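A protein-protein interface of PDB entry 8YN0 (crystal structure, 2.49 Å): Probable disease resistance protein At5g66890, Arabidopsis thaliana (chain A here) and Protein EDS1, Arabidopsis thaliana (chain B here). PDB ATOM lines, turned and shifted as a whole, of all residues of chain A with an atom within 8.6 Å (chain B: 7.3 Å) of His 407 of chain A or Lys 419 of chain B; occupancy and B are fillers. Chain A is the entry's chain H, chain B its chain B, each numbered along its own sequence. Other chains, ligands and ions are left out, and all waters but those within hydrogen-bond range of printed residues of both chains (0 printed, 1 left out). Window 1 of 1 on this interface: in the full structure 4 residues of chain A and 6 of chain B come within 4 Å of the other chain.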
ATOM      1  N   LEU A  65       5.324   5.366   7.462  1.00  0.00           N
ATOM      2  CA  LEU A  65       5.851   6.566   8.104  1.00  0.00           C
ATOM      3  C   LEU A  65       4.923   7.212   9.095  1.00  0.00           C
ATOM      4  O   LEU A  65       3.941   7.802   8.725  1.00  0.00           O
ATOM      5  CB  LEU A  65       6.184   7.576   7.022  1.00  0.00           C
ATOM      6  CG  LEU A  65       7.238   7.279   5.967  1.00  0.00           C
ATOM      7  CD1 LEU A  65       7.003   8.142   4.749  1.00  0.00           C
ATOM      8  CD2 LEU A  65       8.617   7.525   6.539  1.00  0.00           C
ATOM      9  N   PRO A  66       5.257   7.138  10.374  1.00  0.00           N
ATOM     10  CA  PRO A  66       4.317   7.656  11.371  1.00  0.00           C
ATOM     11  C   PRO A  66       4.338   9.177  11.371  1.00  0.00           C
ATOM     12  O   PRO A  66       5.382   9.799  11.183  1.00  0.00           O
ATOM     13  CB  PRO A  66       4.839   7.061  12.680  1.00  0.00           C
ATOM     14  CG  PRO A  66       6.315   6.891  12.408  1.00  0.00           C
ATOM     15  CD  PRO A  66       6.394   6.441  10.995  1.00  0.00           C
ATOM     16  N   GLY A  68       2.586  10.927  13.917  1.00  0.00           N
ATOM     17  CA  GLY A  68       1.989  11.251  15.193  1.00  0.00           C
ATOM     18  C   GLY A  68       2.225  10.129  16.182  1.00  0.00           C
ATOM     19  O   GLY A  68       2.996   9.195  15.921  1.00  0.00           O
ATOM     20  N   LYS A 359      -2.156  14.371  25.878  1.00  0.00           N
ATOM     21  CA  LYS A 359      -0.721  14.629  25.729  1.00  0.00           C
ATOM     22  C   LYS A 359      -0.308  16.084  25.667  1.00  0.00           C
ATOM     23  O   LYS A 359       0.865  16.365  25.928  1.00  0.00           O
ATOM     24  CB  LYS A 359      -0.131  14.017  24.458  1.00  0.00           C
ATOM     25  CG  LYS A 359       1.411  14.096  24.466  1.00  0.00           C
ATOM     26  CD  LYS A 359       2.068  13.830  23.127  1.00  0.00           C
ATOM     27  CE  LYS A 359       2.804  15.067  22.619  1.00  0.00           C
ATOM     28  NZ  LYS A 359       3.363  14.845  21.243  1.00  0.00           N
ATOM     29  N   LYS A 404       6.777  11.285  25.375  1.00  0.00           N
ATOM     30  CA  LYS A 404       7.570  12.389  24.847  1.00  0.00           C
ATOM     31  C   LYS A 404       7.452  12.302  23.325  1.00  0.00           C
ATOM     32  O   LYS A 404       7.376  11.211  22.749  1.00  0.00           O
ATOM     33  CB  LYS A 404       9.084  12.299  25.235  1.00  0.00           C
ATOM     34  CG  LYS A 404      10.116  13.479  24.914  1.00  0.00           C
ATOM     35  CD  LYS A 404      10.251  14.541  25.951  1.00  0.00           C
ATOM     36  CE  LYS A 404      11.377  14.099  26.840  1.00  0.00           C
ATOM     37  NZ  LYS A 404      12.543  14.414  26.054  1.00  0.00           N
ATOM     38  N   THR A 405       7.551  13.437  22.657  1.00  0.00           N
ATOM     39  CA  THR A 405       7.292  13.458  21.226  1.00  0.00           C
ATOM     40  C   THR A 405       8.478  12.923  20.432  1.00  0.00           C
ATOM     41  O   THR A 405       9.635  13.157  20.790  1.00  0.00           O
ATOM     42  CB  THR A 405       6.957  14.880  20.776  1.00  0.00           C
ATOM     43  OG1 THR A 405       5.839  15.368  21.526  1.00  0.00           O
ATOM     44  CG2 THR A 405       6.598  14.932  19.287  1.00  0.00           C
ATOM     45  N   GLU A 406       8.187  12.204  19.343  1.00  0.00           N
ATOM     46  CA  GLU A 406       9.208  11.727  18.408  1.00  0.00           C
ATOM     47  C   GLU A 406       9.245  12.675  17.218  1.00  0.00           C
ATOM     48  O   GLU A 406       8.292  12.728  16.436  1.00  0.00           O
ATOM     49  CB  GLU A 406       8.919  10.302  17.926  1.00  0.00           C
ATOM     50  CG  GLU A 406       9.411   9.211  18.851  1.00  0.00           C
ATOM     51  CD  GLU A 406      10.915   9.238  18.971  1.00  0.00           C
ATOM     52  OE1 GLU A 406      11.439   8.806  20.026  1.00  0.00           O
ATOM     53  OE2 GLU A 406      11.566   9.702  18.000  1.00  0.00           O
ATOM     54  N   HIS A 407      10.348  13.405  17.067  1.00  0.00           N
ATOM     55  CA  HIS A 407      10.447  14.443  16.049  1.00  0.00           C
ATOM     56  C   HIS A 407      11.005  13.876  14.750  1.00  0.00           C
ATOM     57  O   HIS A 407      12.040  13.199  14.741  1.00  0.00           O
ATOM     58  CB  HIS A 407      11.293  15.622  16.549  1.00  0.00           C
ATOM     59  CG  HIS A 407      10.601  16.429  17.607  1.00  0.00           C
ATOM     60  ND1 HIS A 407       9.455  17.162  17.353  1.00  0.00           N
ATOM     61  CD2 HIS A 407      10.849  16.569  18.929  1.00  0.00           C
ATOM     62  CE1 HIS A 407       9.040  17.733  18.470  1.00  0.00           C
ATOM     63  NE2 HIS A 407       9.871  17.391  19.442  1.00  0.00           N
ATOM     64  N   ASN A 408      10.291  14.179  13.680  1.00  0.00           N
ATOM     65  CA  ASN A 408      10.684  13.755  12.366  1.00  0.00           C
ATOM     66  C   ASN A 408      10.048  14.706  11.364  1.00  0.00           C
ATOM     67  O   ASN A 408       9.339  15.602  11.752  1.00  0.00           O
ATOM     68  CB  ASN A 408      10.302  12.298  12.103  1.00  0.00           C
ATOM     69  CG  ASN A 408       8.843  12.044  12.167  1.00  0.00           C
ATOM     70  OD1 ASN A 408       8.114  12.466  11.304  1.00  0.00           O
ATOM     71  ND2 ASN A 408       8.412  11.305  13.166  1.00  0.00           N
ATOM     72  N   LEU A 409      10.306  14.511  10.094  1.00  0.00           N
ATOM     73  CA  LEU A 409       9.773  15.353   9.032  1.00  0.00           C
ATOM     74  C   LEU A 409       8.659  14.697   8.207  1.00  0.00           C
ATOM     75  O   LEU A 409       8.358  15.154   7.148  1.00  0.00           O
ATOM     76  CB  LEU A 409      10.907  15.915   8.199  1.00  0.00           C
ATOM     77  CG  LEU A 409      11.738  16.982   8.904  1.00  0.00           C
ATOM     78  CD1 LEU A 409      12.815  17.500   7.976  1.00  0.00           C
ATOM     79  CD2 LEU A 409      10.877  18.124   9.407  1.00  0.00           C
ATOM     80  N   ASN A 410       8.044  13.648   8.707  1.00  0.00           N
ATOM     81  CA  ASN A 410       7.055  12.872   7.978  1.00  0.00           C
ATOM     82  C   ASN A 410       5.787  13.614   7.521  1.00  0.00           C
ATOM     83  O   ASN A 410       5.269  13.305   6.483  1.00  0.00           O
ATOM     84  CB  ASN A 410       6.732  11.618   8.772  1.00  0.00           C
ATOM     85  CG  ASN A 410       7.889  10.643   8.853  1.00  0.00           C
ATOM     86  OD1 ASN A 410       8.894  10.790   8.180  1.00  0.00           O
ATOM     87  ND2 ASN A 410       7.744   9.636   9.691  1.00  0.00           N
ATOM     88  N   LYS B 386      20.455  10.718  22.948  1.00  0.00           N
ATOM     89  CA  LYS B 386      20.612  11.835  22.101  1.00  0.00           C
ATOM     90  C   LYS B 386      22.060  12.134  21.896  1.00  0.00           C
ATOM     91  O   LYS B 386      22.477  12.398  20.793  1.00  0.00           O
ATOM     92  CB  LYS B 386      19.961  13.018  22.768  1.00  0.00           C
ATOM     93  CG  LYS B 386      18.488  12.882  23.084  1.00  0.00           C
ATOM     94  CD  LYS B 386      18.004  14.144  23.775  1.00  0.00           C
ATOM     95  CE  LYS B 386      16.722  13.922  24.551  1.00  0.00           C
ATOM     96  NZ  LYS B 386      15.553  13.717  23.667  1.00  0.00           N
ATOM     97  N   TRP B 389      23.337   9.344  19.558  1.00  0.00           N
ATOM     98  CA  TRP B 389      22.972   9.487  18.194  1.00  0.00           C
ATOM     99  C   TRP B 389      23.815  10.520  17.592  1.00  0.00           C
ATOM    100  O   TRP B 389      24.356  10.337  16.503  1.00  0.00           O
ATOM    101  CB  TRP B 389      21.527   9.896  18.093  1.00  0.00           C
ATOM    102  CG  TRP B 389      20.994  10.109  16.710  1.00  0.00           C
ATOM    103  CD1 TRP B 389      20.339   9.196  15.909  1.00  0.00           C
ATOM    104  CD2 TRP B 389      21.023  11.341  15.931  1.00  0.00           C
ATOM    105  NE1 TRP B 389      19.988   9.757  14.718  1.00  0.00           N
ATOM    106  CE2 TRP B 389      20.372  11.038  14.667  1.00  0.00           C
ATOM    107  CE3 TRP B 389      21.514  12.606  16.143  1.00  0.00           C
ATOM    108  CZ2 TRP B 389      20.228  11.979  13.679  1.00  0.00           C
ATOM    109  CZ3 TRP B 389      21.365  13.543  15.139  1.00  0.00           C
ATOM    110  CH2 TRP B 389      20.738  13.236  13.939  1.00  0.00           C
ATOM    111  N   ILE B 390      23.977  11.627  18.281  1.00  0.00           N
ATOM    112  CA  ILE B 390      24.875  12.609  17.679  1.00  0.00           C
ATOM    113  C   ILE B 390      26.251  11.992  17.457  1.00  0.00           C
ATOM    114  O   ILE B 390      26.926  12.279  16.464  1.00  0.00           O
ATOM    115  CB  ILE B 390      24.972  13.876  18.551  1.00  0.00           C
ATOM    116  CG1 ILE B 390      23.606  14.551  18.725  1.00  0.00           C
ATOM    117  CG2 ILE B 390      26.012  14.838  17.978  1.00  0.00           C
ATOM    118  CD1 ILE B 390      23.665  15.738  19.705  1.00  0.00           C
ATOM    119  N   TYR B 394      24.906  10.470  13.703  1.00  0.00           N
ATOM    120  CA  TYR B 394      25.045  11.717  12.959  1.00  0.00           C
ATOM    121  C   TYR B 394      26.476  11.920  12.481  1.00  0.00           C
ATOM    122  O   TYR B 394      26.714  12.183  11.295  1.00  0.00           O
ATOM    123  CB  TYR B 394      24.609  12.902  13.814  1.00  0.00           C
ATOM    124  CG  TYR B 394      24.335  14.162  13.016  1.00  0.00           C
ATOM    125  CD1 TYR B 394      23.451  14.150  11.940  1.00  0.00           C
ATOM    126  CD2 TYR B 394      24.950  15.363  13.344  1.00  0.00           C
ATOM    127  CE1 TYR B 394      23.190  15.300  11.216  1.00  0.00           C
ATOM    128  CE2 TYR B 394      24.687  16.521  12.628  1.00  0.00           C
ATOM    129  CZ  TYR B 394      23.802  16.479  11.568  1.00  0.00           C
ATOM    130  OH  TYR B 394      23.539  17.628  10.864  1.00  0.00           O
ATOM    131  N   PHE B 409      25.457  20.022   9.405  1.00  0.00           N
ATOM    132  CA  PHE B 409      24.468  20.801  10.144  1.00  0.00           C
ATOM    133  C   PHE B 409      24.290  22.181   9.533  1.00  0.00           C
ATOM    134  O   PHE B 409      23.171  22.707   9.482  1.00  0.00           O
ATOM    135  CB  PHE B 409      24.883  20.931  11.607  1.00  0.00           C
ATOM    136  CG  PHE B 409      23.790  21.440  12.502  1.00  0.00           C
ATOM    137  CD1 PHE B 409      23.586  22.808  12.671  1.00  0.00           C
ATOM    138  CD2 PHE B 409      22.967  20.541  13.183  1.00  0.00           C
ATOM    139  CE1 PHE B 409      22.582  23.276  13.502  1.00  0.00           C
ATOM    140  CE2 PHE B 409      21.962  20.991  14.022  1.00  0.00           C
ATOM    141  CZ  PHE B 409      21.765  22.361  14.184  1.00  0.00           C
ATOM    142  N   SER B 412      21.729  22.578   5.892  1.00  0.00           N
ATOM    143  CA  SER B 412      20.812  21.748   6.666  1.00  0.00           C
ATOM    144  C   SER B 412      19.860  21.058   5.681  1.00  0.00           C
ATOM    145  O   SER B 412      18.677  21.379   5.582  1.00  0.00           O
ATOM    146  CB  SER B 412      20.112  22.605   7.720  1.00  0.00           C
ATOM    147  OG  SER B 412      19.494  21.838   8.733  1.00  0.00           O
ATOM    148  N   GLU B 414      19.181  17.484   5.096  1.00  0.00           N
ATOM    149  CA  GLU B 414      18.534  16.197   5.275  1.00  0.00           C
ATOM    150  C   GLU B 414      17.727  16.157   6.568  1.00  0.00           C
ATOM    151  O   GLU B 414      17.871  16.992   7.461  1.00  0.00           O
ATOM    152  CB  GLU B 414      19.576  15.066   5.283  1.00  0.00           C
ATOM    153  CG  GLU B 414      20.413  14.932   4.016  1.00  0.00           C
ATOM    154  CD  GLU B 414      21.339  13.700   4.004  1.00  0.00           C
ATOM    155  OE1 GLU B 414      21.624  13.091   5.067  1.00  0.00           O
ATOM    156  OE2 GLU B 414      21.800  13.347   2.903  1.00  0.00           O
ATOM    157  N   GLU B 415      16.858  15.154   6.666  1.00  0.00           N
ATOM    158  CA  GLU B 415      16.087  15.010   7.887  1.00  0.00           C
ATOM    159  C   GLU B 415      17.013  14.814   9.072  1.00  0.00           C
ATOM    160  O   GLU B 415      16.736  15.301  10.174  1.00  0.00           O
ATOM    161  CB  GLU B 415      15.098  13.850   7.774  1.00  0.00           C
ATOM    162  CG  GLU B 415      13.917  14.027   8.678  1.00  0.00           C
ATOM    163  CD  GLU B 415      12.913  12.925   8.557  1.00  0.00           C
ATOM    164  OE1 GLU B 415      12.753  12.417   7.436  1.00  0.00           O
ATOM    165  OE2 GLU B 415      12.276  12.577   9.580  1.00  0.00           O
ATOM    166  N   ASN B 416      18.135  14.127   8.862  1.00  0.00           N
ATOM    167  CA  ASN B 416      19.056  13.918   9.971  1.00  0.00           C
ATOM    168  C   ASN B 416      19.553  15.243  10.525  1.00  0.00           C
ATOM    169  O   ASN B 416      19.748  15.371  11.732  1.00  0.00           O
ATOM    170  CB  ASN B 416      20.219  13.036   9.539  1.00  0.00           C
ATOM    171  CG  ASN B 416      19.871  11.573   9.643  1.00  0.00           C
ATOM    172  OD1 ASN B 416      18.785  11.216  10.139  1.00  0.00           O
ATOM    173  ND2 ASN B 416      20.773  10.711   9.176  1.00  0.00           N
ATOM    174  N   ASP B 417      19.754  16.238   9.662  1.00  0.00           N
ATOM    175  CA  ASP B 417      20.163  17.551  10.149  1.00  0.00           C
ATOM    176  C   ASP B 417      19.099  18.148  11.057  1.00  0.00           C
ATOM    177  O   ASP B 417      19.420  18.783  12.076  1.00  0.00           O
ATOM    178  CB  ASP B 417      20.440  18.490   8.980  1.00  0.00           C
ATOM    179  CG  ASP B 417      21.462  17.942   8.019  1.00  0.00           C
ATOM    180  OD1 ASP B 417      22.501  17.402   8.478  1.00  0.00           O
ATOM    181  OD2 ASP B 417      21.228  18.084   6.797  1.00  0.00           O
ATOM    182  N   PHE B 418      17.826  17.968  10.694  1.00  0.00           N
ATOM    183  CA  PHE B 418      16.738  18.473  11.520  1.00  0.00           C
ATOM    184  C   PHE B 418      16.710  17.745  12.858  1.00  0.00           C
ATOM    185  O   PHE B 418      16.514  18.364  13.917  1.00  0.00           O
ATOM    186  CB  PHE B 418      15.407  18.319  10.771  1.00  0.00           C
ATOM    187  CG  PHE B 418      14.182  18.472  11.642  1.00  0.00           C
ATOM    188  CD1 PHE B 418      13.720  19.733  12.008  1.00  0.00           C
ATOM    189  CD2 PHE B 418      13.495  17.353  12.101  1.00  0.00           C
ATOM    190  CE1 PHE B 418      12.601  19.870  12.835  1.00  0.00           C
ATOM    191  CE2 PHE B 418      12.357  17.484  12.916  1.00  0.00           C
ATOM    192  CZ  PHE B 418      11.912  18.736  13.282  1.00  0.00           C
ATOM    193  N   LYS B 419      16.909  16.426  12.830  1.00  0.00           N
ATOM    194  CA  LYS B 419      16.914  15.669  14.071  1.00  0.00           C
ATOM    195  C   LYS B 419      18.063  16.132  14.948  1.00  0.00           C
ATOM    196  O   LYS B 419      17.924  16.240  16.178  1.00  0.00           O
ATOM    197  CB  LYS B 419      16.999  14.173  13.771  1.00  0.00           C
ATOM    198  CG  LYS B 419      15.739  13.624  13.069  1.00  0.00           C
ATOM    199  CD  LYS B 419      15.620  12.109  13.121  1.00  0.00           C
ATOM    200  CE  LYS B 419      14.537  11.596  12.156  1.00  0.00           C
ATOM    201  NZ  LYS B 419      14.270  10.117  12.271  1.00  0.00           N
ATOM    202  N   ALA B 420      19.189  16.468  14.310  1.00  0.00           N
ATOM    203  CA  ALA B 420      20.347  16.974  15.022  1.00  0.00           C
ATOM    204  C   ALA B 420      20.021  18.303  15.691  1.00  0.00           C
ATOM    205  O   ALA B 420      20.333  18.511  16.874  1.00  0.00           O
ATOM    206  CB  ALA B 420      21.519  17.107  14.048  1.00  0.00           C
ATOM    207  N   ASN B 421      19.347  19.199  14.960  1.00  0.00           N
ATOM    208  CA  ASN B 421      18.990  20.482  15.546  1.00  0.00           C
ATOM    209  C   ASN B 421      18.019  20.303  16.712  1.00  0.00           C
ATOM    210  O   ASN B 421      18.120  21.008  17.734  1.00  0.00           O
ATOM    211  CB  ASN B 421      18.400  21.397  14.491  1.00  0.00           C
ATOM    212  CG  ASN B 421      18.085  22.769  15.044  1.00  0.00           C
ATOM    213  OD1 ASN B 421      18.799  23.273  15.904  1.00  0.00           O
ATOM    214  ND2 ASN B 421      16.988  23.370  14.579  1.00  0.00           N
ATOM    215  N   VAL B 422      17.085  19.347  16.585  1.00  0.00           N
ATOM    216  CA  VAL B 422      16.082  19.129  17.633  1.00  0.00           C
ATOM    217  C   VAL B 422      16.727  18.553  18.893  1.00  0.00           C
ATOM    218  O   VAL B 422      16.429  18.988  20.015  1.00  0.00           O
ATOM    219  CB  VAL B 422      14.945  18.226  17.119  1.00  0.00           C
ATOM    220  CG1 VAL B 422      14.050  17.766  18.268  1.00  0.00           C
ATOM    221  CG2 VAL B 422      14.123  18.972  16.097  1.00  0.00           C
ATOM    222  N   LYS B 423      17.571  17.524  18.733  1.00  0.00           N
ATOM    223  CA  LYS B 423      18.378  17.027  19.845  1.00  0.00           C
ATOM    224  C   LYS B 423      19.156  18.165  20.492  1.00  0.00           C
ATOM    225  O   LYS B 423      19.254  18.246  21.732  1.00  0.00           O
ATOM    226  CB  LYS B 423      19.356  15.959  19.354  1.00  0.00           C
ATOM    227  CG  LYS B 423      18.960  14.496  19.529  1.00  0.00           C
ATOM    228  CD  LYS B 423      18.113  13.944  18.397  1.00  0.00           C
ATOM    229  CE  LYS B 423      18.064  12.431  18.463  1.00  0.00           C
ATOM    230  NZ  LYS B 423      16.807  11.878  17.902  1.00  0.00           N
ATOM    231  N   ARG B 424      19.725  19.048  19.660  1.00  0.00           N
ATOM    232  CA  ARG B 424      20.534  20.149  20.175  1.00  0.00           C
ATOM    233  C   ARG B 424      19.701  21.073  21.054  1.00  0.00           C
ATOM    234  O   ARG B 424      20.143  21.469  22.135  1.00  0.00           O
ATOM    235  CB  ARG B 424      21.180  20.919  19.011  1.00  0.00           C
ATOM    236  CG  ARG B 424      21.927  22.203  19.434  1.00  0.00           C
ATOM    237  CD  ARG B 424      21.919  23.237  18.309  1.00  0.00           C
ATOM    238  NE  ARG B 424      20.553  23.570  17.913  1.00  0.00           N
ATOM    239  CZ  ARG B 424      19.774  24.412  18.582  1.00  0.00           C
ATOM    240  NH1 ARG B 424      20.239  25.050  19.653  1.00  0.00           N
ATOM    241  NH2 ARG B 424      18.542  24.637  18.164  1.00  0.00           N
ATOM    242  N   ALA B 425      18.467  21.380  20.630  1.00  0.00           N
ATOM    243  CA  ALA B 425      17.595  22.239  21.439  1.00  0.00           C
ATOM    244  C   ALA B 425      17.126  21.527  22.712  1.00  0.00           C
ATOM    245  O   ALA B 425      17.044  22.145  23.782  1.00  0.00           O
ATOM    246  CB  ALA B 425      16.397  22.725  20.618  1.00  0.00           C
ATOM    247  N   GLU B 426      16.835  20.229  22.632  1.00  0.00           N
ATOM    248  CA  GLU B 426      16.352  19.521  23.819  1.00  0.00           C
ATOM    249  C   GLU B 426      17.441  19.443  24.874  1.00  0.00           C
ATOM    250  O   GLU B 426      17.187  19.642  26.077  1.00  0.00           O
ATOM    251  CB  GLU B 426      15.864  18.112  23.446  1.00  0.00           C
ATOM    252  CG  GLU B 426      14.492  18.101  22.801  1.00  0.00           C
ATOM    253  CD  GLU B 426      14.143  16.786  22.093  1.00  0.00           C
ATOM    254  OE1 GLU B 426      12.937  16.477  22.010  1.00  0.00           O
ATOM    255  OE2 GLU B 426      15.048  16.056  21.615  1.00  0.00           O
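Printed residues of chain A that touch a printed residue of chain B: Lys 404, His 407, Asn 408 and Leu 409.
Along chain A the printed residues that touch a printed residue of chain B span positions 404 to 409.
Of the 19 printed residues of chain B, 6 touch a printed residue of chain A.
Hydrophobic or aromatic side chains of chain B that line the printed part of chain A: Phe 418 and Val 422.
Among the printed residues, no Asp or Glu carboxylate lies within 4 Å of a Lys or Arg side-chain nitrogen of the other chain.
The backbone NH (N) of Leu 409 of chain A sits at hydrogen-bond distance from the side-chain carboxylate (OE2) of Glu 415 of chain B (2.8 Å).
The side-chain amino group (NZ) of Lys 386 of chain B lies within salt-bridge range of the side-chain carboxylate (OE2) of Glu 426 of chain B (3.2 Å).
N of Asn 410 of chain A is in hydrogen-bond range of OD1 of Asn 408 of chain A (2.9 Å).
Among the printed residues, merely in contact across the chains: Lys 404 of chain A with Lys 386 of chain B (3.9 Å), His 407 of chain A with Lys 419 of chain B (3.9 Å), His 407 of chain A with Val 422 of chain B (3.5 Å), His 407 of chain A with Glu 426 of chain B (3.7 Å), Asn 408 of chain A with Glu 415 of chain B (3.2 Å), Asn 408 of chain A with Phe 418 of chain B (3.7 Å) and Leu 409 of chain A with Phe 418 of chain B (3.7 Å).
Of chain B, only Lys 419 (3.9 Å), Val 422 (3.5 Å) and Glu 426 (3.7 Å) come within 4 Å of His 407 of chain A.
No residue of chain A comes within 4 Å of Ala 420 of chain B.
Of the printed residues of chain A, Phe 418 of chain B touches Asn 408 and Leu 409.
Printed residues of chain A within 4 Å of Glu 415 of chain B: Asn 408 (3.2 Å) and Leu 409 (2.8 Å).
Thr 405 of chain A touches none of the printed residues of chain B.
Gly 68 of chain A touches none of the printed residues of chain B.
The nearest residue of chain A that does not touch Lys 419 of chain B is Asn 408 of chain A (4.3 Å).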
